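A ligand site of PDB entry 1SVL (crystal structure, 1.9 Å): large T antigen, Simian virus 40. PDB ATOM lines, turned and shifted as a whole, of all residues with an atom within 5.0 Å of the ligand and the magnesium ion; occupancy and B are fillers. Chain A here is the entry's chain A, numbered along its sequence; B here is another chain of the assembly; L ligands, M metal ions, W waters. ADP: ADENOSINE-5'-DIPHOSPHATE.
The side-chain amino group (NZ) of Lys 182 sits at hydrogen-bond distance from the backbone carbonyl oxygen (O) of Pro 177 (2.8 Å).
OG1 of Thr 183 lies close to OE2 of Glu 223 (3.3 Å).
NZ of Lys 182 lies within hydrogen-bond range of OD1 of Asn 279 (3.3 Å).
OD2 of Asp 179 is in salt-bridge range of NZ of Lys 168 of chain B, at 3.7 Å.
The backbone carbonyl oxygen of Leu 303 sits at hydrogen-bond distance from the indole nitrogen of Trp 143.
The side-chain hydroxyl (OG) of Ser 180 lies within hydrogen-bond range of the backbone carbonyl oxygen (O) of Pro 177, at 2.7 Å.
Water W2 is bound to the magnesium ion.
O2B of the ligand is bound to the magnesium ion, at 2.0 Å.
The magnesium ion is bound by water W3.
The magnesium ion is bound by water W1 (2.2 Å).
Water W4 binds the magnesium ion, 2.3 Å away.
The magnesium ion is bound by OG1 of Thr 183, 2.3 Å away.
The magnesium ion has six donor atoms within binding distance.
The side-chain amino group of Lys 182 is in salt-bridge range of an oxygen (O1B) of the ligand (2.9 Å).
An oxygen (O3B) of the ligand sits at hydrogen-bond distance from the backbone NH (N) of Asp 179 (2.7 Å).
O1B of the ligand sits at hydrogen-bond distance from N of Ser 180 (3.0 Å).
The backbone carbonyl oxygen (O) of Ser 180 is in hydrogen-bond range of a nitrogen (N6) of the ligand (3.1 Å).
O1B of the ligand sits at hydrogen-bond distance from N of Lys 182 (3.1 Å).
The backbone NH (N) of Thr 184 is in hydrogen-bond range of an oxygen (O1A) of the ligand.
N1 of the ligand is in hydrogen-bond range of N of Lys 300 (2.8 Å).
The side-chain hydroxyl of Thr 184 lies within hydrogen-bond range of an oxygen (O1A) of the ligand, at 2.6 Å.
A nitrogen (N6) of the ligand sits at hydrogen-bond distance from the backbone carbonyl oxygen (O) of Arg 298, at 2.9 Å.
The backbone NH (N) of Thr 183 is in hydrogen-bond range of an oxygen (O1A) of the ligand (3.3 Å).
N of Gly 181 is in hydrogen-bond range of O1B of the ligand, at 3.1 Å.
Trp 143 touches the ligand (CH2 to C8, 3.8 Å).
CD1 of Leu 147 touches N6 of the ligand (3.7 Å).
Pro 177 touches the ligand (O to O1B, 3.8 Å).
CA of Ile 178 touches O3B of the ligand, 3.5 Å away.
Pro 299 touches the ligand (CA to N1, 3.2 Å).
CD1 of Leu 303 touches N6 of the ligand (3.3 Å).
Leu 307 touches the ligand (CD1 to O2', 3.3 Å).
Leu 314 touches the ligand (CD2 to O2', 3.6 Å).
Lys 168 of chain B touches the ligand.
Within 4 Å of the ligand: Trp 143, Leu 147, Pro 177, Ile 178, Asp 179, Ser 180, Gly 181, Lys 182, Thr 183, Thr 184, Arg 298, Pro 299, Lys 300, Leu 303, Leu 307, Leu 314 and Lys 168 of chain B.
Merely in contact with the magnesium ion: Glu 223 (3.5 Å).
Within 4 Å of the magnesium ion: Thr 183 and Glu 223.
The nearest printed residue that does not touch the magnesium ion is Lys 182 (4.8 Å).
Water W1 lies within hydrogen-bond range of O2A of the ligand and NZ of Lys 168 of chain B.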
ATOM      1  N   TRP A 143      21.277  -3.478  19.745  1.00  0.00           N
ATOM      2  CA  TRP A 143      21.766  -4.611  18.955  1.00  0.00           C
ATOM      3  C   TRP A 143      21.696  -4.259  17.470  1.00  0.00           C
ATOM      4  O   TRP A 143      22.648  -4.481  16.710  1.00  0.00           O
ATOM      5  CB  TRP A 143      20.910  -5.851  19.226  1.00  0.00           C
ATOM      6  CG  TRP A 143      21.461  -7.124  18.622  1.00  0.00           C
ATOM      7  CD1 TRP A 143      22.373  -7.979  19.175  1.00  0.00           C
ATOM      8  CD2 TRP A 143      21.149  -7.650  17.337  1.00  0.00           C
ATOM      9  NE1 TRP A 143      22.638  -9.016  18.304  1.00  0.00           N
ATOM     10  CE2 TRP A 143      21.902  -8.836  17.168  1.00  0.00           C
ATOM     11  CE3 TRP A 143      20.300  -7.244  16.292  1.00  0.00           C
ATOM     12  CZ2 TRP A 143      21.837  -9.610  16.009  1.00  0.00           C
ATOM     13  CZ3 TRP A 143      20.230  -8.016  15.146  1.00  0.00           C
ATOM     14  CH2 TRP A 143      20.995  -9.186  15.009  1.00  0.00           C
ATOM     15  N   LEU A 147      24.291  -3.887  13.863  1.00  0.00           N
ATOM     16  CA  LEU A 147      24.117  -4.783  12.728  1.00  0.00           C
ATOM     17  C   LEU A 147      24.735  -4.230  11.458  1.00  0.00           C
ATOM     18  O   LEU A 147      25.244  -4.993  10.634  1.00  0.00           O
ATOM     19  CB  LEU A 147      22.623  -5.049  12.480  1.00  0.00           C
ATOM     20  CG  LEU A 147      22.266  -6.117  11.429  1.00  0.00           C
ATOM     21  CD1 LEU A 147      22.692  -7.488  11.928  1.00  0.00           C
ATOM     22  CD2 LEU A 147      20.773  -6.141  11.180  1.00  0.00           C
ATOM     23  N   PRO A 177      26.003 -13.514   3.435  1.00  0.00           N
ATOM     24  CA  PRO A 177      25.871 -14.920   3.837  1.00  0.00           C
ATOM     25  C   PRO A 177      24.599 -15.172   4.654  1.00  0.00           C
ATOM     26  O   PRO A 177      23.943 -14.229   5.125  1.00  0.00           O
ATOM     27  CB  PRO A 177      27.126 -15.167   4.680  1.00  0.00           C
ATOM     28  CG  PRO A 177      28.110 -14.184   4.132  1.00  0.00           C
ATOM     29  CD  PRO A 177      27.272 -12.947   3.919  1.00  0.00           C
ATOM     30  N   ILE A 178      24.263 -16.446   4.823  1.00  0.00           N
ATOM     31  CA  ILE A 178      23.093 -16.814   5.598  1.00  0.00           C
ATOM     32  C   ILE A 178      23.293 -16.328   7.035  1.00  0.00           C
ATOM     33  O   ILE A 178      24.402 -16.338   7.560  1.00  0.00           O
ATOM     34  CB  ILE A 178      22.894 -18.352   5.615  1.00  0.00           C
ATOM     35  CG1 ILE A 178      22.737 -18.886   4.194  1.00  0.00           C
ATOM     36  CG2 ILE A 178      21.666 -18.698   6.427  1.00  0.00           C
ATOM     37  CD1 ILE A 178      21.403 -18.548   3.542  1.00  0.00           C
ATOM     38  N   ASP A 179      22.204 -15.910   7.670  1.00  0.00           N
ATOM     39  CA  ASP A 179      22.252 -15.428   9.032  1.00  0.00           C
ATOM     40  C   ASP A 179      23.133 -14.195   9.252  1.00  0.00           C
ATOM     41  O   ASP A 179      23.892 -14.132  10.204  1.00  0.00           O
ATOM     42  CB  ASP A 179      22.706 -16.575   9.962  1.00  0.00           C
ATOM     43  CG  ASP A 179      21.717 -17.736   9.972  1.00  0.00           C
ATOM     44  OD1 ASP A 179      22.091 -18.845  10.417  1.00  0.00           O
ATOM     45  OD2 ASP A 179      20.561 -17.549   9.526  1.00  0.00           O
ATOM     46  N   SER A 180      23.014 -13.206   8.371  1.00  0.00           N
ATOM     47  CA  SER A 180      23.803 -11.977   8.536  1.00  0.00           C
ATOM     48  C   SER A 180      22.895 -10.796   8.881  1.00  0.00           C
ATOM     49  O   SER A 180      23.368  -9.685   9.180  1.00  0.00           O
ATOM     50  CB  SER A 180      24.658 -11.689   7.294  1.00  0.00           C
ATOM     51  OG  SER A 180      23.893 -11.735   6.107  1.00  0.00           O
ATOM     52  N   GLY A 181      21.583 -11.018   8.848  1.00  0.00           N
ATOM     53  CA  GLY A 181      20.658  -9.965   9.203  1.00  0.00           C
ATOM     54  C   GLY A 181      19.727  -9.454   8.125  1.00  0.00           C
ATOM     55  O   GLY A 181      18.866  -8.611   8.400  1.00  0.00           O
ATOM     56  N   LYS A 182      19.879  -9.949   6.904  1.00  0.00           N
ATOM     57  CA  LYS A 182      19.066  -9.517   5.775  1.00  0.00           C
ATOM     58  C   LYS A 182      17.551  -9.600   6.033  1.00  0.00           C
ATOM     59  O   LYS A 182      16.829  -8.604   5.876  1.00  0.00           O
ATOM     60  CB  LYS A 182      19.413 -10.356   4.537  1.00  0.00           C
ATOM     61  CG  LYS A 182      20.896 -10.344   4.145  1.00  0.00           C
ATOM     62  CD  LYS A 182      21.120 -11.042   2.798  1.00  0.00           C
ATOM     63  CE  LYS A 182      20.751 -12.539   2.854  1.00  0.00           C
ATOM     64  NZ  LYS A 182      21.586 -13.272   3.843  1.00  0.00           N
ATOM     65  N   THR A 183      17.069 -10.780   6.429  1.00  0.00           N
ATOM     66  CA  THR A 183      15.640 -10.937   6.693  1.00  0.00           C
ATOM     67  C   THR A 183      15.192 -10.214   7.964  1.00  0.00           C
ATOM     68  O   THR A 183      14.081  -9.686   8.022  1.00  0.00           O
ATOM     69  CB  THR A 183      15.280 -12.428   6.758  1.00  0.00           C
ATOM     70  OG1 THR A 183      15.481 -13.008   5.456  1.00  0.00           O
ATOM     71  CG2 THR A 183      13.806 -12.629   7.159  1.00  0.00           C
ATOM     72  N   THR A 184      16.065 -10.183   8.955  1.00  0.00           N
ATOM     73  CA  THR A 184      15.745  -9.510  10.212  1.00  0.00           C
ATOM     74  C   THR A 184      15.417  -8.047   9.905  1.00  0.00           C
ATOM     75  O   THR A 184      14.391  -7.514  10.357  1.00  0.00           O
ATOM     76  CB  THR A 184      16.942  -9.563  11.196  1.00  0.00           C
ATOM     77  OG1 THR A 184      17.277 -10.937  11.466  1.00  0.00           O
ATOM     78  CG2 THR A 184      16.593  -8.861  12.513  1.00  0.00           C
ATOM     79  N   GLU A 223      11.842 -11.805  -0.925  1.00  0.00           N
ATOM     80  CA  GLU A 223      12.610 -12.603   0.030  1.00  0.00           C
ATOM     81  C   GLU A 223      13.423 -13.774  -0.517  1.00  0.00           C
ATOM     82  O   GLU A 223      12.933 -14.570  -1.317  1.00  0.00           O
ATOM     83  CB  GLU A 223      11.667 -13.093   1.152  1.00  0.00           C
ATOM     84  CG  GLU A 223      12.299 -13.975   2.237  1.00  0.00           C
ATOM     85  CD  GLU A 223      13.217 -13.219   3.186  1.00  0.00           C
ATOM     86  OE1 GLU A 223      13.622 -13.842   4.195  1.00  0.00           O
ATOM     87  OE2 GLU A 223      13.535 -12.038   2.938  1.00  0.00           O
ATOM     88  N   ASP A 224      14.667 -13.862  -0.059  1.00  0.00           N
ATOM     89  CA  ASP A 224      15.604 -14.932  -0.423  1.00  0.00           C
ATOM     90  C   ASP A 224      15.557 -15.369  -1.884  1.00  0.00           C
ATOM     91  O   ASP A 224      15.267 -16.539  -2.177  1.00  0.00           O
ATOM     92  CB  ASP A 224      15.350 -16.132   0.484  1.00  0.00           C
ATOM     93  CG  ASP A 224      16.359 -17.246   0.290  1.00  0.00           C
ATOM     94  OD1 ASP A 224      17.566 -16.940   0.218  1.00  0.00           O
ATOM     95  OD2 ASP A 224      15.939 -18.424   0.229  1.00  0.00           O
ATOM     96  N   ASN A 279      21.344 -14.104  -0.822  1.00  0.00           N
ATOM     97  CA  ASN A 279      22.581 -14.673  -0.326  1.00  0.00           C
ATOM     98  C   ASN A 279      23.697 -14.307  -1.310  1.00  0.00           C
ATOM     99  O   ASN A 279      23.529 -13.395  -2.125  1.00  0.00           O
ATOM    100  CB  ASN A 279      22.459 -16.198  -0.171  1.00  0.00           C
ATOM    101  CG  ASN A 279      21.457 -16.585   0.918  1.00  0.00           C
ATOM    102  OD1 ASN A 279      21.419 -15.982   1.990  1.00  0.00           O
ATOM    103  ND2 ASN A 279      20.647 -17.605   0.644  1.00  0.00           N
ATOM    104  N   ARG A 298      27.030  -8.902   7.197  1.00  0.00           N
ATOM    105  CA  ARG A 298      28.074  -9.844   7.584  1.00  0.00           C
ATOM    106  C   ARG A 298      27.888 -10.405   8.976  1.00  0.00           C
ATOM    107  O   ARG A 298      27.558  -9.677   9.922  1.00  0.00           O
ATOM    108  CB  ARG A 298      29.449  -9.171   7.476  1.00  0.00           C
ATOM    109  CG  ARG A 298      29.756  -8.612   6.103  1.00  0.00           C
ATOM    110  CD  ARG A 298      31.201  -8.199   5.956  1.00  0.00           C
ATOM    111  NE  ARG A 298      31.487  -7.765   4.585  1.00  0.00           N
ATOM    112  CZ  ARG A 298      32.705  -7.531   4.111  1.00  0.00           C
ATOM    113  NH1 ARG A 298      33.767  -7.689   4.893  1.00  0.00           N
ATOM    114  NH2 ARG A 298      32.861  -7.139   2.856  1.00  0.00           N
ATOM    115  N   PRO A 299      28.080 -11.718   9.138  1.00  0.00           N
ATOM    116  CA  PRO A 299      27.926 -12.332  10.453  1.00  0.00           C
ATOM    117  C   PRO A 299      28.947 -11.728  11.407  1.00  0.00           C
ATOM    118  O   PRO A 299      30.040 -11.364  10.986  1.00  0.00           O
ATOM    119  CB  PRO A 299      28.186 -13.809  10.183  1.00  0.00           C
ATOM    120  CG  PRO A 299      27.713 -13.976   8.765  1.00  0.00           C
ATOM    121  CD  PRO A 299      28.288 -12.756   8.103  1.00  0.00           C
ATOM    122  N   LYS A 300      28.576 -11.615  12.679  1.00  0.00           N
ATOM    123  CA  LYS A 300      29.475 -11.080  13.695  1.00  0.00           C
ATOM    124  C   LYS A 300      29.368 -11.905  14.968  1.00  0.00           C
ATOM    125  O   LYS A 300      28.278 -12.098  15.501  1.00  0.00           O
ATOM    126  CB  LYS A 300      29.142  -9.618  13.988  1.00  0.00           C
ATOM    127  CG  LYS A 300      29.359  -8.684  12.808  1.00  0.00           C
ATOM    128  CD  LYS A 300      28.952  -7.249  13.133  1.00  0.00           C
ATOM    129  CE  LYS A 300      29.078  -6.320  11.931  1.00  0.00           C
ATOM    130  NZ  LYS A 300      28.602  -4.949  12.267  1.00  0.00           N
ATOM    131  N   LEU A 303      27.523 -10.476  17.846  1.00  0.00           N
ATOM    132  CA  LEU A 303      26.078 -10.367  17.641  1.00  0.00           C
ATOM    133  C   LEU A 303      25.397 -11.674  18.039  1.00  0.00           C
ATOM    134  O   LEU A 303      24.329 -11.661  18.654  1.00  0.00           O
ATOM    135  CB  LEU A 303      25.770 -10.039  16.184  1.00  0.00           C
ATOM    136  CG  LEU A 303      26.168  -8.637  15.715  1.00  0.00           C
ATOM    137  CD1 LEU A 303      25.680  -8.402  14.281  1.00  0.00           C
ATOM    138  CD2 LEU A 303      25.586  -7.602  16.658  1.00  0.00           C
ATOM    139  N   LYS A 304      26.015 -12.792  17.695  1.00  0.00           N
ATOM    140  CA  LYS A 304      25.470 -14.108  18.020  1.00  0.00           C
ATOM    141  C   LYS A 304      25.566 -14.359  19.518  1.00  0.00           C
ATOM    142  O   LYS A 304      24.569 -14.664  20.167  1.00  0.00           O
ATOM    143  CB  LYS A 304      26.230 -15.189  17.262  1.00  0.00           C
ATOM    144  CG  LYS A 304      25.811 -16.613  17.613  1.00  0.00           C
ATOM    145  CD  LYS A 304      26.696 -17.652  16.906  1.00  0.00           C
ATOM    146  CE  LYS A 304      28.166 -17.523  17.317  1.00  0.00           C
ATOM    147  NZ  LYS A 304      29.046 -18.524  16.630  1.00  0.00           N
ATOM    148  N   LEU A 307      23.202 -12.244  21.694  1.00  0.00           N
ATOM    149  CA  LEU A 307      21.844 -12.775  21.697  1.00  0.00           C
ATOM    150  C   LEU A 307      21.675 -13.978  22.626  1.00  0.00           C
ATOM    151  O   LEU A 307      20.682 -14.090  23.337  1.00  0.00           O
ATOM    152  CB  LEU A 307      21.439 -13.166  20.269  1.00  0.00           C
ATOM    153  CG  LEU A 307      21.090 -11.987  19.363  1.00  0.00           C
ATOM    154  CD1 LEU A 307      20.910 -12.497  17.945  1.00  0.00           C
ATOM    155  CD2 LEU A 307      19.824 -11.292  19.852  1.00  0.00           C
ATOM    156  N   LEU A 314      15.054 -12.363  20.896  1.00  0.00           N
ATOM    157  CA  LEU A 314      14.462 -13.250  19.895  1.00  0.00           C
ATOM    158  C   LEU A 314      13.126 -13.798  20.343  1.00  0.00           C
ATOM    159  O   LEU A 314      12.214 -13.946  19.537  1.00  0.00           O
ATOM    160  CB  LEU A 314      15.403 -14.405  19.587  1.00  0.00           C
ATOM    161  CG  LEU A 314      16.729 -14.035  18.919  1.00  0.00           C
ATOM    162  CD1 LEU A 314      17.643 -15.246  18.902  1.00  0.00           C
ATOM    163  CD2 LEU A 314      16.450 -13.552  17.518  1.00  0.00           C
ATOM    164  N   ILE A 319      14.262  -7.631  17.758  1.00  0.00           N
ATOM    165  CA  ILE A 319      15.167  -7.200  16.703  1.00  0.00           C
ATOM    166  C   ILE A 319      14.584  -7.199  15.297  1.00  0.00           C
ATOM    167  O   ILE A 319      15.180  -6.624  14.388  1.00  0.00           O
ATOM    168  CB  ILE A 319      16.477  -8.015  16.694  1.00  0.00           C
ATOM    169  CG1 ILE A 319      16.191  -9.501  16.525  1.00  0.00           C
ATOM    170  CG2 ILE A 319      17.258  -7.749  17.988  1.00  0.00           C
ATOM    171  CD1 ILE A 319      17.446 -10.342  16.411  1.00  0.00           C
ATOM    172  N   GLN A 320      13.440  -7.830  15.090  1.00  0.00           N
ATOM    173  CA  GLN A 320      12.846  -7.811  13.767  1.00  0.00           C
ATOM    174  C   GLN A 320      11.556  -7.007  13.778  1.00  0.00           C
ATOM    175  O   GLN A 320      10.724  -7.108  12.876  1.00  0.00           O
ATOM    176  CB  GLN A 320      12.578  -9.235  13.258  1.00  0.00           C
ATOM    177  CG  GLN A 320      11.875 -10.187  14.211  1.00  0.00           C
ATOM    178  CD  GLN A 320      12.810 -10.794  15.256  1.00  0.00           C
ATOM    179  OE1 GLN A 320      12.847 -10.338  16.399  1.00  0.00           O
ATOM    180  NE2 GLN A 320      13.583 -11.804  14.846  1.00  0.00           N
ATOM    181  N   PRO B 167      11.983 -17.364  15.462  1.00  0.00           N
ATOM    182  CA  PRO B 167      12.325 -17.483  14.036  1.00  0.00           C
ATOM    183  C   PRO B 167      13.493 -18.446  13.785  1.00  0.00           C
ATOM    184  O   PRO B 167      14.511 -18.370  14.460  1.00  0.00           O
ATOM    185  CB  PRO B 167      12.665 -16.048  13.639  1.00  0.00           C
ATOM    186  CG  PRO B 167      11.749 -15.247  14.534  1.00  0.00           C
ATOM    187  CD  PRO B 167      11.893 -15.952  15.871  1.00  0.00           C
ATOM    188  N   LYS B 168      13.309 -19.372  12.843  1.00  0.00           N
ATOM    189  CA  LYS B 168      14.316 -20.381  12.499  1.00  0.00           C
ATOM    190  C   LYS B 168      14.579 -21.418  13.599  1.00  0.00           C
ATOM    191  O   LYS B 168      15.411 -22.315  13.432  1.00  0.00           O
ATOM    192  CB  LYS B 168      15.641 -19.712  12.115  1.00  0.00           C
ATOM    193  CG  LYS B 168      15.608 -18.898  10.826  1.00  0.00           C
ATOM    194  CD  LYS B 168      16.884 -18.087  10.686  1.00  0.00           C
ATOM    195  CE  LYS B 168      16.914 -17.263   9.410  1.00  0.00           C
ATOM    196  NZ  LYS B 168      17.186 -18.070   8.185  1.00  0.00           N
ATOM    197  N   SER B 254       9.940 -16.211   9.851  1.00  0.00           N
ATOM    198  CA  SER B 254      10.515 -14.870  10.012  1.00  0.00           C
ATOM    199  C   SER B 254       9.531 -13.846   9.447  1.00  0.00           C
ATOM    200  O   SER B 254       9.118 -12.918  10.119  1.00  0.00           O
ATOM    201  CB  SER B 254      11.837 -14.740   9.259  1.00  0.00           C
ATOM    202  OG  SER B 254      12.879 -15.360   9.979  1.00  0.00           O
HETATM  203  PB  ADP L   1      19.573 -13.988   6.768  1.00  0.00           P
HETATM  204  O1B ADP L   1      20.619 -12.963   6.576  1.00  0.00           O
HETATM  205  O2B ADP L   1      18.194 -13.567   6.107  1.00  0.00           O
HETATM  206  O3B ADP L   1      20.032 -15.290   6.192  1.00  0.00           O
HETATM  207  PA  ADP L   1      18.209 -13.483   9.309  1.00  0.00           P
HETATM  208  O1A ADP L   1      18.262 -12.011   9.277  1.00  0.00           O
HETATM  209  O2A ADP L   1      16.855 -13.922   8.960  1.00  0.00           O
HETATM  210  O3A ADP L   1      19.272 -14.125   8.296  1.00  0.00           O
HETATM  211  O5' ADP L   1      18.520 -14.031  10.749  1.00  0.00           O
HETATM  212  C5' ADP L   1      19.561 -14.959  11.064  1.00  0.00           C
HETATM  213  C4' ADP L   1      19.532 -15.219  12.574  1.00  0.00           C
HETATM  214  O4' ADP L   1      20.913 -15.178  12.956  1.00  0.00           O
HETATM  215  C3' ADP L   1      18.829 -14.137  13.420  1.00  0.00           C
HETATM  216  O3' ADP L   1      17.548 -14.555  13.931  1.00  0.00           O
HETATM  217  C2' ADP L   1      19.805 -13.797  14.539  1.00  0.00           C
HETATM  218  O2' ADP L   1      19.428 -14.477  15.758  1.00  0.00           O
HETATM  219  C1' ADP L   1      21.167 -14.177  13.953  1.00  0.00           C
HETATM  220  N9  ADP L   1      21.931 -13.054  13.255  1.00  0.00           N
HETATM  221  C8  ADP L   1      21.384 -12.038  12.517  1.00  0.00           C
HETATM  222  N7  ADP L   1      22.346 -11.252  12.052  1.00  0.00           N
HETATM  223  C5  ADP L   1      23.509 -11.708  12.470  1.00  0.00           C
HETATM  224  C6  ADP L   1      24.864 -11.336  12.313  1.00  0.00           C
HETATM  225  N6  ADP L   1      25.199 -10.242  11.593  1.00  0.00           N
HETATM  226  N1  ADP L   1      25.833 -12.086  12.911  1.00  0.00           N
HETATM  227  C2  ADP L   1      25.562 -13.194  13.649  1.00  0.00           C
HETATM  228  N3  ADP L   1      24.285 -13.565  13.809  1.00  0.00           N
HETATM  229  C4  ADP L   1      23.245 -12.878  13.245  1.00  0.00           C
HETATM  230 MG    MG M   1      16.996 -14.644   4.864  1.00  0.00          MG
HETATM  231  O   HOH W   1      16.397 -15.593   6.758  1.00  0.00           O
HETATM  232  O   HOH W   2      18.505 -15.802   4.313  1.00  0.00           O
HETATM  233  O   HOH W   3      17.235 -13.510   3.066  1.00  0.00           O
HETATM  234  O   HOH W   4      15.316 -15.662   3.745  1.00  0.00           O
